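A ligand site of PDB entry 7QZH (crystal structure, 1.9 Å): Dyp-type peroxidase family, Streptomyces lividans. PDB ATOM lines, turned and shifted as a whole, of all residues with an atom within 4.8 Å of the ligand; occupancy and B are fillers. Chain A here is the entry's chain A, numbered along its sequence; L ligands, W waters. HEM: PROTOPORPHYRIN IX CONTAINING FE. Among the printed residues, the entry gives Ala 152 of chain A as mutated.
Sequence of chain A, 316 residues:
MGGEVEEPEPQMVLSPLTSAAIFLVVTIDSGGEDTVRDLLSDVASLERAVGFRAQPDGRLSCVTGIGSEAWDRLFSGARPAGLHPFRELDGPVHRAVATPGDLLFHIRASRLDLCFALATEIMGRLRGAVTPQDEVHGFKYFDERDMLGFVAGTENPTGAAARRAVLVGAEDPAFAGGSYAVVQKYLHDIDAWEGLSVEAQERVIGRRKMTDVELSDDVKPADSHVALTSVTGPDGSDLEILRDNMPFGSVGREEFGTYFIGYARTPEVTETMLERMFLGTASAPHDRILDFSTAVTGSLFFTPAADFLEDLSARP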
ATOM      1  N   ASP A 146      -7.275  -3.400  26.148  1.00  0.00           N
ATOM      2  CA  ASP A 146      -8.643  -3.021  25.906  1.00  0.00           C
ATOM      3  C   ASP A 146      -9.200  -2.455  27.226  1.00  0.00           C
ATOM      4  O   ASP A 146      -8.492  -2.284  28.231  1.00  0.00           O
ATOM      5  CB  ASP A 146      -9.434  -4.210  25.353  1.00  0.00           C
ATOM      6  CG  ASP A 146      -9.679  -5.384  26.263  1.00  0.00           C
ATOM      7  OD1 ASP A 146      -9.420  -5.254  27.485  1.00  0.00           O
ATOM      8  OD2 ASP A 146     -10.015  -6.457  25.722  1.00  0.00           O
ATOM      9  N   LEU A 148     -11.180  -3.800  29.312  1.00  0.00           N
ATOM     10  CA  LEU A 148     -11.178  -4.780  30.402  1.00  0.00           C
ATOM     11  C   LEU A 148      -9.774  -5.005  31.030  1.00  0.00           C
ATOM     12  O   LEU A 148      -9.660  -5.720  32.028  1.00  0.00           O
ATOM     13  CB  LEU A 148     -11.749  -6.100  29.880  1.00  0.00           C
ATOM     14  CG  LEU A 148     -13.177  -6.005  29.319  1.00  0.00           C
ATOM     15  CD1 LEU A 148     -13.678  -7.375  28.884  1.00  0.00           C
ATOM     16  CD2 LEU A 148     -14.119  -5.328  30.284  1.00  0.00           C
ATOM     17  N   PHE A 150      -7.113  -6.287  29.368  1.00  0.00           N
ATOM     18  CA  PHE A 150      -6.411  -7.395  28.731  1.00  0.00           C
ATOM     19  C   PHE A 150      -5.835  -6.930  27.399  1.00  0.00           C
ATOM     20  O   PHE A 150      -6.403  -6.059  26.689  1.00  0.00           O
ATOM     21  CB  PHE A 150      -7.360  -8.593  28.535  1.00  0.00           C
ATOM     22  CG  PHE A 150      -7.589  -9.434  29.759  1.00  0.00           C
ATOM     23  CD1 PHE A 150      -8.399  -8.968  30.779  1.00  0.00           C
ATOM     24  CD2 PHE A 150      -7.050 -10.692  29.863  1.00  0.00           C
ATOM     25  CE1 PHE A 150      -8.573  -9.706  31.933  1.00  0.00           C
ATOM     26  CE2 PHE A 150      -7.217 -11.433  31.023  1.00  0.00           C
ATOM     27  CZ  PHE A 150      -7.999 -10.954  32.033  1.00  0.00           C
ATOM     28  N   VAL A 151      -4.703  -7.561  27.007  1.00  0.00           N
ATOM     29  CA  VAL A 151      -4.098  -7.291  25.694  1.00  0.00           C
ATOM     30  C   VAL A 151      -5.070  -7.762  24.614  1.00  0.00           C
ATOM     31  O   VAL A 151      -5.607  -8.874  24.707  1.00  0.00           O
ATOM     32  CB  VAL A 151      -2.702  -7.944  25.554  1.00  0.00           C
ATOM     33  CG1 VAL A 151      -2.104  -7.749  24.175  1.00  0.00           C
ATOM     34  CG2 VAL A 151      -1.735  -7.456  26.632  1.00  0.00           C
ATOM     35  N   ALA A 152      -5.228  -6.952  23.559  1.00  0.00           N
ATOM     36  CA  ALA A 152      -6.166  -7.258  22.485  1.00  0.00           C
ATOM     37  C   ALA A 152      -5.399  -7.294  21.154  1.00  0.00           C
ATOM     38  O   ALA A 152      -4.755  -6.310  20.736  1.00  0.00           O
ATOM     39  CB  ALA A 152      -7.240  -6.173  22.431  1.00  0.00           C
ATOM     40  N   GLY A 153      -5.474  -8.451  20.476  1.00  0.00           N
ATOM     41  CA  GLY A 153      -4.957  -8.617  19.117  1.00  0.00           C
ATOM     42  C   GLY A 153      -3.894  -9.705  19.004  1.00  0.00           C
ATOM     43  O   GLY A 153      -3.489 -10.049  17.886  1.00  0.00           O
ATOM     44  N   THR A 154      -3.475 -10.282  20.132  1.00  0.00           N
ATOM     45  CA  THR A 154      -2.308 -11.178  20.202  1.00  0.00           C
ATOM     46  C   THR A 154      -2.360 -12.296  19.161  1.00  0.00           C
ATOM     47  O   THR A 154      -1.350 -12.549  18.503  1.00  0.00           O
ATOM     48  CB  THR A 154      -2.191 -11.780  21.617  1.00  0.00           C
ATOM     49  OG1 THR A 154      -2.233 -10.666  22.520  1.00  0.00           O
ATOM     50  CG2 THR A 154      -0.937 -12.589  21.878  1.00  0.00           C
ATOM     51  N   GLU A 155      -3.488 -12.988  19.033  1.00  0.00           N
ATOM     52  CA  GLU A 155      -3.579 -14.185  18.188  1.00  0.00           C
ATOM     53  C   GLU A 155      -4.161 -13.869  16.824  1.00  0.00           C
ATOM     54  O   GLU A 155      -4.592 -14.793  16.118  1.00  0.00           O
ATOM     55  CB  GLU A 155      -4.388 -15.265  18.906  1.00  0.00           C
ATOM     56  CG  GLU A 155      -3.636 -15.899  20.074  1.00  0.00           C
ATOM     57  CD  GLU A 155      -2.377 -16.616  19.632  1.00  0.00           C
ATOM     58  OE1 GLU A 155      -2.522 -17.550  18.851  1.00  0.00           O
ATOM     59  OE2 GLU A 155      -1.290 -16.198  20.044  1.00  0.00           O
ATOM     60  N   ASN A 156      -4.200 -12.586  16.402  1.00  0.00           N
ATOM     61  CA  ASN A 156      -4.511 -12.291  15.005  1.00  0.00           C
ATOM     62  C   ASN A 156      -3.532 -13.061  14.092  1.00  0.00           C
ATOM     63  O   ASN A 156      -2.341 -13.080  14.383  1.00  0.00           O
ATOM     64  CB  ASN A 156      -4.412 -10.811  14.682  1.00  0.00           C
ATOM     65  CG  ASN A 156      -5.714 -10.070  14.893  1.00  0.00           C
ATOM     66  OD1 ASN A 156      -6.776 -10.634  14.679  1.00  0.00           O
ATOM     67  ND2 ASN A 156      -5.611  -8.807  15.321  1.00  0.00           N
ATOM     68  N   GLN A 184     -19.594  -4.665  15.652  1.00  0.00           N
ATOM     69  CA  GLN A 184     -20.501  -4.580  16.781  1.00  0.00           C
ATOM     70  C   GLN A 184     -19.883  -3.610  17.785  1.00  0.00           C
ATOM     71  O   GLN A 184     -18.729  -3.755  18.161  1.00  0.00           O
ATOM     72  CB  GLN A 184     -20.672  -5.915  17.514  1.00  0.00           C
ATOM     73  CG  GLN A 184     -21.262  -7.053  16.659  1.00  0.00           C
ATOM     74  CD  GLN A 184     -21.345  -8.285  17.528  1.00  0.00           C
ATOM     75  OE1 GLN A 184     -20.312  -8.865  17.897  1.00  0.00           O
ATOM     76  NE2 GLN A 184     -22.563  -8.634  17.957  1.00  0.00           N
ATOM     77  N   TYR A 186     -19.694  -2.577  21.517  1.00  0.00           N
ATOM     78  CA  TYR A 186     -19.997  -3.147  22.817  1.00  0.00           C
ATOM     79  C   TYR A 186     -19.779  -2.094  23.907  1.00  0.00           C
ATOM     80  O   TYR A 186     -18.805  -1.355  23.800  1.00  0.00           O
ATOM     81  CB  TYR A 186     -19.061  -4.301  23.122  1.00  0.00           C
ATOM     82  CG  TYR A 186     -19.419  -5.583  22.424  1.00  0.00           C
ATOM     83  CD1 TYR A 186     -20.290  -6.491  23.001  1.00  0.00           C
ATOM     84  CD2 TYR A 186     -18.803  -5.916  21.232  1.00  0.00           C
ATOM     85  CE1 TYR A 186     -20.586  -7.704  22.401  1.00  0.00           C
ATOM     86  CE2 TYR A 186     -19.153  -7.096  20.566  1.00  0.00           C
ATOM     87  CZ  TYR A 186     -20.017  -7.999  21.170  1.00  0.00           C
ATOM     88  OH  TYR A 186     -20.336  -9.180  20.532  1.00  0.00           O
ATOM     89  N   HIS A 188     -19.301  -1.956  28.154  1.00  0.00           N
ATOM     90  CA  HIS A 188     -18.905  -2.822  29.229  1.00  0.00           C
ATOM     91  C   HIS A 188     -19.531  -2.323  30.542  1.00  0.00           C
ATOM     92  O   HIS A 188     -19.607  -1.130  30.764  1.00  0.00           O
ATOM     93  CB  HIS A 188     -17.403  -2.930  29.371  1.00  0.00           C
ATOM     94  CG  HIS A 188     -16.785  -3.580  28.176  1.00  0.00           C
ATOM     95  ND1 HIS A 188     -17.005  -4.893  27.855  1.00  0.00           N
ATOM     96  CD2 HIS A 188     -15.912  -3.046  27.257  1.00  0.00           C
ATOM     97  CE1 HIS A 188     -16.314  -5.169  26.722  1.00  0.00           C
ATOM     98  NE2 HIS A 188     -15.645  -4.020  26.320  1.00  0.00           N
ATOM     99  N   ILE A 205     -11.664 -14.718  30.178  1.00  0.00           N
ATOM    100  CA  ILE A 205     -11.007 -14.459  28.912  1.00  0.00           C
ATOM    101  C   ILE A 205     -10.341 -15.739  28.383  1.00  0.00           C
ATOM    102  O   ILE A 205     -10.470 -16.058  27.197  1.00  0.00           O
ATOM    103  CB  ILE A 205      -9.990 -13.315  29.048  1.00  0.00           C
ATOM    104  CG1 ILE A 205     -10.659 -12.011  29.529  1.00  0.00           C
ATOM    105  CG2 ILE A 205      -9.183 -13.117  27.739  1.00  0.00           C
ATOM    106  CD1 ILE A 205     -11.627 -11.408  28.544  1.00  0.00           C
ATOM    107  N   ARG A 207      -6.816 -16.197  29.149  1.00  0.00           N
ATOM    108  CA  ARG A 207      -5.404 -15.815  29.101  1.00  0.00           C
ATOM    109  C   ARG A 207      -5.055 -15.135  30.415  1.00  0.00           C
ATOM    110  O   ARG A 207      -5.970 -14.580  31.068  1.00  0.00           O
ATOM    111  CB  ARG A 207      -5.072 -14.867  27.948  1.00  0.00           C
ATOM    112  CG  ARG A 207      -5.573 -15.336  26.569  1.00  0.00           C
ATOM    113  CD  ARG A 207      -5.191 -14.439  25.427  1.00  0.00           C
ATOM    114  NE  ARG A 207      -3.758 -14.458  25.177  1.00  0.00           N
ATOM    115  CZ  ARG A 207      -3.167 -15.289  24.320  1.00  0.00           C
ATOM    116  NH1 ARG A 207      -3.907 -16.097  23.565  1.00  0.00           N
ATOM    117  NH2 ARG A 207      -1.861 -15.323  24.241  1.00  0.00           N
ATOM    118  N   ASP A 212      -0.262 -12.104  29.400  1.00  0.00           N
ATOM    119  CA  ASP A 212      -0.918 -12.432  28.149  1.00  0.00           C
ATOM    120  C   ASP A 212      -0.514 -13.840  27.639  1.00  0.00           C
ATOM    121  O   ASP A 212      -0.596 -14.125  26.434  1.00  0.00           O
ATOM    122  CB  ASP A 212      -0.630 -11.392  27.066  1.00  0.00           C
ATOM    123  CG  ASP A 212      -1.554 -11.470  25.842  1.00  0.00           C
ATOM    124  OD1 ASP A 212      -2.707 -11.997  25.966  1.00  0.00           O
ATOM    125  OD2 ASP A 212      -1.137 -10.994  24.781  1.00  0.00           O
ATOM    126  N   HIS A 225     -13.788 -16.913  26.723  1.00  0.00           N
ATOM    127  CA  HIS A 225     -13.839 -16.274  25.432  1.00  0.00           C
ATOM    128  C   HIS A 225     -12.921 -16.936  24.389  1.00  0.00           C
ATOM    129  O   HIS A 225     -13.342 -17.161  23.235  1.00  0.00           O
ATOM    130  CB  HIS A 225     -13.493 -14.800  25.601  1.00  0.00           C
ATOM    131  CG  HIS A 225     -13.617 -14.010  24.332  1.00  0.00           C
ATOM    132  ND1 HIS A 225     -14.767 -13.956  23.607  1.00  0.00           N
ATOM    133  CD2 HIS A 225     -12.673 -13.289  23.680  1.00  0.00           C
ATOM    134  CE1 HIS A 225     -14.581 -13.202  22.514  1.00  0.00           C
ATOM    135  NE2 HIS A 225     -13.267 -12.778  22.536  1.00  0.00           N
ATOM    136  N   VAL A 226     -11.671 -17.230  24.766  1.00  0.00           N
ATOM    137  CA  VAL A 226     -10.744 -17.854  23.833  1.00  0.00           C
ATOM    138  C   VAL A 226     -11.211 -19.276  23.442  1.00  0.00           C
ATOM    139  O   VAL A 226     -10.994 -19.668  22.287  1.00  0.00           O
ATOM    140  CB  VAL A 226      -9.303 -17.810  24.358  1.00  0.00           C
ATOM    141  CG1 VAL A 226      -8.350 -18.733  23.650  1.00  0.00           C
ATOM    142  CG2 VAL A 226      -8.777 -16.385  24.308  1.00  0.00           C
ATOM    143  N   THR A 229     -14.231 -18.884  20.834  1.00  0.00           N
ATOM    144  CA  THR A 229     -13.871 -18.277  19.572  1.00  0.00           C
ATOM    145  C   THR A 229     -12.789 -19.048  18.832  1.00  0.00           C
ATOM    146  O   THR A 229     -12.288 -18.557  17.812  1.00  0.00           O
ATOM    147  CB  THR A 229     -13.520 -16.785  19.729  1.00  0.00           C
ATOM    148  OG1 THR A 229     -12.379 -16.621  20.603  1.00  0.00           O
ATOM    149  CG2 THR A 229     -14.705 -16.001  20.219  1.00  0.00           C
ATOM    150  N   SER A 230     -12.406 -20.204  19.368  1.00  0.00           N
ATOM    151  CA  SER A 230     -11.472 -21.124  18.731  1.00  0.00           C
ATOM    152  C   SER A 230     -12.311 -22.135  17.943  1.00  0.00           C
ATOM    153  O   SER A 230     -13.129 -22.849  18.568  1.00  0.00           O
ATOM    154  CB  SER A 230     -10.625 -21.858  19.750  1.00  0.00           C
ATOM    155  OG  SER A 230      -9.739 -20.969  20.399  1.00  0.00           O
ATOM    156  N   ILE A 241     -10.053 -15.198  11.859  1.00  0.00           N
ATOM    157  CA  ILE A 241     -10.476 -13.884  11.395  1.00  0.00           C
ATOM    158  C   ILE A 241      -9.419 -12.868  11.803  1.00  0.00           C
ATOM    159  O   ILE A 241      -8.568 -13.122  12.630  1.00  0.00           O
ATOM    160  CB  ILE A 241     -11.881 -13.526  11.932  1.00  0.00           C
ATOM    161  CG1 ILE A 241     -11.915 -13.304  13.448  1.00  0.00           C
ATOM    162  CG2 ILE A 241     -12.917 -14.531  11.457  1.00  0.00           C
ATOM    163  CD1 ILE A 241     -13.240 -12.724  13.954  1.00  0.00           C
ATOM    164  N   ARG A 243      -9.013  -9.197  13.530  1.00  0.00           N
ATOM    165  CA  ARG A 243      -9.746  -8.282  14.402  1.00  0.00           C
ATOM    166  C   ARG A 243      -8.942  -7.004  14.631  1.00  0.00           C
ATOM    167  O   ARG A 243      -7.708  -7.067  14.733  1.00  0.00           O
ATOM    168  CB  ARG A 243     -10.031  -8.974  15.742  1.00  0.00           C
ATOM    169  CG  ARG A 243     -10.847 -10.234  15.602  1.00  0.00           C
ATOM    170  CD  ARG A 243     -10.760 -11.112  16.815  1.00  0.00           C
ATOM    171  NE  ARG A 243      -9.415 -11.699  16.967  1.00  0.00           N
ATOM    172  CZ  ARG A 243      -8.577 -11.434  17.971  1.00  0.00           C
ATOM    173  NH1 ARG A 243      -8.945 -10.616  18.986  1.00  0.00           N
ATOM    174  NH2 ARG A 243      -7.396 -12.049  17.986  1.00  0.00           N
ATOM    175  N   ASN A 245     -10.117  -4.453  17.098  1.00  0.00           N
ATOM    176  CA  ASN A 245     -10.913  -3.924  18.169  1.00  0.00           C
ATOM    177  C   ASN A 245     -10.276  -2.639  18.710  1.00  0.00           C
ATOM    178  O   ASN A 245      -9.059  -2.578  18.950  1.00  0.00           O
ATOM    179  CB  ASN A 245     -11.092  -4.911  19.303  1.00  0.00           C
ATOM    180  CG  ASN A 245     -11.814  -6.195  18.927  1.00  0.00           C
ATOM    181  OD1 ASN A 245     -12.132  -6.430  17.761  1.00  0.00           O
ATOM    182  ND2 ASN A 245     -12.038  -7.023  19.925  1.00  0.00           N
ATOM    183  N   THR A 258     -15.820  -1.301  23.735  1.00  0.00           N
ATOM    184  CA  THR A 258     -14.937  -1.948  22.758  1.00  0.00           C
ATOM    185  C   THR A 258     -15.670  -1.880  21.413  1.00  0.00           C
ATOM    186  O   THR A 258     -16.820  -2.356  21.333  1.00  0.00           O
ATOM    187  CB  THR A 258     -14.683  -3.405  23.094  1.00  0.00           C
ATOM    188  OG1 THR A 258     -13.970  -3.480  24.313  1.00  0.00           O
ATOM    189  CG2 THR A 258     -13.882  -4.121  22.011  1.00  0.00           C
ATOM    190  N   PHE A 260     -15.831  -3.586  18.099  1.00  0.00           N
ATOM    191  CA  PHE A 260     -15.388  -4.809  17.486  1.00  0.00           C
ATOM    192  C   PHE A 260     -15.528  -4.657  15.957  1.00  0.00           C
ATOM    193  O   PHE A 260     -16.596  -4.292  15.459  1.00  0.00           O
ATOM    194  CB  PHE A 260     -16.225  -6.007  17.958  1.00  0.00           C
ATOM    195  CG  PHE A 260     -15.953  -7.262  17.181  1.00  0.00           C
ATOM    196  CD1 PHE A 260     -14.820  -8.004  17.425  1.00  0.00           C
ATOM    197  CD2 PHE A 260     -16.764  -7.618  16.111  1.00  0.00           C
ATOM    198  CE1 PHE A 260     -14.531  -9.137  16.682  1.00  0.00           C
ATOM    199  CE2 PHE A 260     -16.451  -8.738  15.314  1.00  0.00           C
ATOM    200  CZ  PHE A 260     -15.336  -9.486  15.609  1.00  0.00           C
ATOM    201  N   THR A 270     -17.033 -15.826  10.877  1.00  0.00           N
ATOM    202  CA  THR A 270     -17.368 -14.870  11.932  1.00  0.00           C
ATOM    203  C   THR A 270     -18.710 -15.204  12.578  1.00  0.00           C
ATOM    204  O   THR A 270     -18.871 -15.079  13.796  1.00  0.00           O
ATOM    205  CB  THR A 270     -17.395 -13.425  11.359  1.00  0.00           C
ATOM    206  OG1 THR A 270     -16.223 -13.242  10.564  1.00  0.00           O
ATOM    207  CG2 THR A 270     -17.460 -12.392  12.454  1.00  0.00           C
ATOM    208  N   MET A 273     -18.479 -18.097  15.015  1.00  0.00           N
ATOM    209  CA  MET A 273     -17.966 -17.604  16.311  1.00  0.00           C
ATOM    210  C   MET A 273     -19.071 -16.909  17.117  1.00  0.00           C
ATOM    211  O   MET A 273     -19.177 -17.149  18.326  1.00  0.00           O
ATOM    212  CB  MET A 273     -16.788 -16.661  16.083  1.00  0.00           C
ATOM    213  CG  MET A 273     -15.578 -17.335  15.544  1.00  0.00           C
ATOM    214  SD  MET A 273     -14.290 -16.187  15.108  1.00  0.00           S
ATOM    215  CE  MET A 273     -12.970 -17.275  14.583  1.00  0.00           C
ATOM    216  N   LEU A 274     -19.846 -16.021  16.459  1.00  0.00           N
ATOM    217  CA  LEU A 274     -20.903 -15.309  17.137  1.00  0.00           C
ATOM    218  C   LEU A 274     -21.966 -16.259  17.685  1.00  0.00           C
ATOM    219  O   LEU A 274     -22.509 -16.026  18.785  1.00  0.00           O
ATOM    220  CB  LEU A 274     -21.512 -14.291  16.166  1.00  0.00           C
ATOM    221  CG  LEU A 274     -20.726 -13.009  15.931  1.00  0.00           C
ATOM    222  CD1 LEU A 274     -21.376 -12.230  14.791  1.00  0.00           C
ATOM    223  CD2 LEU A 274     -20.681 -12.151  17.191  1.00  0.00           C
ATOM    224  N   MET A 277     -20.704 -17.802  20.796  1.00  0.00           N
ATOM    225  CA  MET A 277     -20.717 -16.840  21.890  1.00  0.00           C
ATOM    226  C   MET A 277     -22.114 -16.622  22.503  1.00  0.00           C
ATOM    227  O   MET A 277     -22.247 -16.573  23.727  1.00  0.00           O
ATOM    228  CB  MET A 277     -20.126 -15.494  21.443  1.00  0.00           C
ATOM    229  CG  MET A 277     -18.620 -15.558  21.100  1.00  0.00           C
ATOM    230  SD  MET A 277     -18.033 -13.969  20.469  1.00  0.00           S
ATOM    231  CE  MET A 277     -18.427 -12.824  21.797  1.00  0.00           C
ATOM    232  N   ILE A 289     -17.651 -13.496  28.533  1.00  0.00           N
ATOM    233  CA  ILE A 289     -17.374 -12.100  28.266  1.00  0.00           C
ATOM    234  C   ILE A 289     -18.684 -11.312  28.106  1.00  0.00           C
ATOM    235  O   ILE A 289     -18.742 -10.136  28.460  1.00  0.00           O
ATOM    236  CB  ILE A 289     -16.383 -11.901  27.070  1.00  0.00           C
ATOM    237  CG1 ILE A 289     -15.444 -10.704  27.277  1.00  0.00           C
ATOM    238  CG2 ILE A 289     -17.096 -11.833  25.734  1.00  0.00           C
ATOM    239  CD1 ILE A 289     -14.390 -10.526  26.225  1.00  0.00           C
ATOM    240  N   SER A 293     -20.552  -7.363  28.887  1.00  0.00           N
ATOM    241  CA  SER A 293     -20.432  -6.690  27.596  1.00  0.00           C
ATOM    242  C   SER A 293     -21.782  -6.798  26.865  1.00  0.00           C
ATOM    243  O   SER A 293     -22.230  -7.897  26.634  1.00  0.00           O
ATOM    244  CB  SER A 293     -19.355  -7.280  26.720  1.00  0.00           C
ATOM    245  OG  SER A 293     -18.174  -7.513  27.439  1.00  0.00           O
HETATM  246  CHA HEM L   1      -9.391 -13.024  21.355  1.00  0.00           C
HETATM  247  CHB HEM L   1     -11.426  -9.331  23.781  1.00  0.00           C
HETATM  248  CHC HEM L   1     -15.432  -9.643  20.972  1.00  0.00           C
HETATM  249  CHD HEM L   1     -13.228 -13.124  18.372  1.00  0.00           C
HETATM  250  C1A HEM L   1      -9.615 -11.988  22.262  1.00  0.00           C
HETATM  251  C2A HEM L   1      -8.695 -11.650  23.343  1.00  0.00           C
HETATM  252  C3A HEM L   1      -9.292 -10.584  24.063  1.00  0.00           C
HETATM  253  C4A HEM L   1     -10.552 -10.268  23.417  1.00  0.00           C
HETATM  254  CMA HEM L   1      -8.757  -9.838  25.248  1.00  0.00           C
HETATM  255  CAA HEM L   1      -7.378 -12.425  23.551  1.00  0.00           C
HETATM  256  CBA HEM L   1      -6.194 -11.780  22.839  1.00  0.00           C
HETATM  257  CGA HEM L   1      -6.357 -11.776  21.336  1.00  0.00           C
HETATM  258  O1A HEM L   1      -6.920 -10.765  20.845  1.00  0.00           O
HETATM  259  O2A HEM L   1      -5.968 -12.790  20.723  1.00  0.00           O
HETATM  260  C1B HEM L   1     -12.661  -9.114  23.213  1.00  0.00           C
HETATM  261  C2B HEM L   1     -13.613  -8.072  23.743  1.00  0.00           C
HETATM  262  C3B HEM L   1     -14.743  -8.113  22.926  1.00  0.00           C
HETATM  263  C4B HEM L   1     -14.528  -9.256  21.937  1.00  0.00           C
HETATM  264  CMB HEM L   1     -13.270  -7.093  24.842  1.00  0.00           C
HETATM  265  CAB HEM L   1     -15.919  -7.351  23.247  1.00  0.00           C
HETATM  266  CBB HEM L   1     -16.929  -8.111  23.531  1.00  0.00           C
HETATM  267  C1C HEM L   1     -15.216 -10.628  20.005  1.00  0.00           C
HETATM  268  C2C HEM L   1     -16.152 -11.118  19.053  1.00  0.00           C
HETATM  269  C3C HEM L   1     -15.513 -12.134  18.313  1.00  0.00           C
HETATM  270  C4C HEM L   1     -14.170 -12.270  18.867  1.00  0.00           C
HETATM  271  CMC HEM L   1     -17.516 -10.612  18.862  1.00  0.00           C
HETATM  272  CAC HEM L   1     -15.977 -12.957  17.181  1.00  0.00           C
HETATM  273  CBC HEM L   1     -17.076 -12.760  16.543  1.00  0.00           C
HETATM  274  C1D HEM L   1     -12.016 -13.322  19.010  1.00  0.00           C
HETATM  275  C2D HEM L   1     -11.056 -14.332  18.472  1.00  0.00           C
HETATM  276  C3D HEM L   1      -9.971 -14.348  19.327  1.00  0.00           C
HETATM  277  C4D HEM L   1     -10.286 -13.345  20.368  1.00  0.00           C
HETATM  278  CMD HEM L   1     -11.245 -15.173  17.225  1.00  0.00           C
HETATM  279  CAD HEM L   1      -8.826 -15.218  19.078  1.00  0.00           C
HETATM  280  CBD HEM L   1      -9.087 -16.559  19.814  1.00  0.00           C
HETATM  281  CGD HEM L   1      -7.856 -17.492  19.657  1.00  0.00           C
HETATM  282  O1D HEM L   1      -7.797 -18.176  18.634  1.00  0.00           O
HETATM  283  O2D HEM L   1      -6.870 -17.504  20.449  1.00  0.00           O
HETATM  284  NA  HEM L   1     -10.716 -11.120  22.328  1.00  0.00           N
HETATM  285  NB  HEM L   1     -13.254  -9.743  22.193  1.00  0.00           N
HETATM  286  NC  HEM L   1     -14.067 -11.293  19.867  1.00  0.00           N
HETATM  287  ND  HEM L   1     -11.522 -12.763  20.122  1.00  0.00           N
HETATM  288 FE   HEM L   1     -12.412 -11.356  21.208  1.00  0.00          FE
HETATM  289  O   HOH W   1      -8.978  -8.356  21.078  1.00  0.00           O
HETATM  290  O   HOH W   2     -11.388  -9.498  19.720  1.00  0.00           O
HETATM  291  O   HOH W   3      -9.731 -18.087  16.881  1.00  0.00           O
HETATM  292  O   HOH W   4      -5.312 -18.613  17.879  1.00  0.00           O
HETATM  293  O   HOH W   5      -5.076 -19.178  20.675  1.00  0.00           O
HETATM  294  O   HOH W   6      -6.223 -15.335  22.143  1.00  0.00           O
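Asp 146 touches the ligand (OD2 to CMB, 3.4 Å).
Phe 150 touches the ligand (CB to CMA, 3.8 Å).
Val 151 touches the ligand (O to CMA, 3.3 Å).
Ala 152 touches the ligand.
Thr 154 touches the ligand.
Gln 184 touches the ligand (OE1 to CMC, 3.4 Å).
Tyr 186 touches the ligand.
Arg 207 touches the ligand (CD to CAA, 3.5 Å).
CG1 of Val 226 touches O2D of the ligand, at 3.7 Å.
Thr 229 touches the ligand.
Ser 230 touches the ligand.
Asn 245 touches the ligand (ND2 to NB, 3.7 Å).
Thr 258 touches the ligand (OG1 to CMB, 3.7 Å).
Phe 260 touches the ligand.
CE of Met 273 touches CMD of the ligand, 3.8 Å away.
CG of Leu 274 touches CBC of the ligand, 3.7 Å away.
Met 277 touches the ligand.
Ile 289 touches the ligand.
Hydrophobic or aromatic side chains within 4 Å of the ligand: Phe 150, Tyr 186, His 225, Val 226, Phe 260, Met 273, Leu 274, Met 277 and Ile 289.
FE of the ligand is bound by NE2 of His 225, at 2.1 Å.
The guanidinium group (NH1) of Arg 243 lies within salt-bridge range of an oxygen (O1A) of the ligand (2.8 Å).
The backbone NH (N) of Gly 153 sits at hydrogen-bond distance from an oxygen (O1A) of the ligand, 2.8 Å away.
The backbone NH (N) of Glu 155 is in hydrogen-bond range of an oxygen (O2A) of the ligand.
O of His 225 is in hydrogen-bond range of OG1 of Thr 229 (2.9 Å).
OD1 of Asp 146 sits at hydrogen-bond distance from N of Phe 150 (3.2 Å).
The side-chain carboxylate (OD1) of Asp 146 is in hydrogen-bond range of the backbone NH (N) of Leu 148 (2.9 Å).
The backbone carbonyl oxygen of Gln 184 lies within hydrogen-bond range of the backbone NH of Phe 260 (2.9 Å).
The side-chain amide oxygen (OE1) of Gln 184 is in hydrogen-bond range of the side-chain hydroxyl (OH) of Tyr 186, at 2.7 Å.
The side-chain carboxylate (OD2) of Asp 212 is in hydrogen-bond range of the side-chain hydroxyl (OG1) of Thr 154 (2.5 Å).
The side-chain hydroxyl (OG) of Ser 230 sits at hydrogen-bond distance from the backbone carbonyl oxygen (O) of Val 226, at 2.6 Å.
O of Ile 205 lies within hydrogen-bond range of N of Val 226, 3.0 Å away.
Water W2 bridges the side-chain amide nitrogen of Asn 245 (2.6 Å) and the guanidinium group of Arg 243 (2.8 Å).
Water W3 bridges an oxygen (O1D) of the ligand (2.6 Å) and the backbone carbonyl oxygen of Thr 229 (2.8 Å).
Water W4 lies within hydrogen-bond range of O1D of the ligand (2.6 Å) and OE1 of Glu 155 (3.1 Å).
Water W6 lies within hydrogen-bond range of NH1 of Arg 207 (2.8 Å) and O2D of the ligand (2.8 Å).
Water W1 bridges NH1 of Arg 243 (3.1 Å) and O1A of the ligand (3.2 Å).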
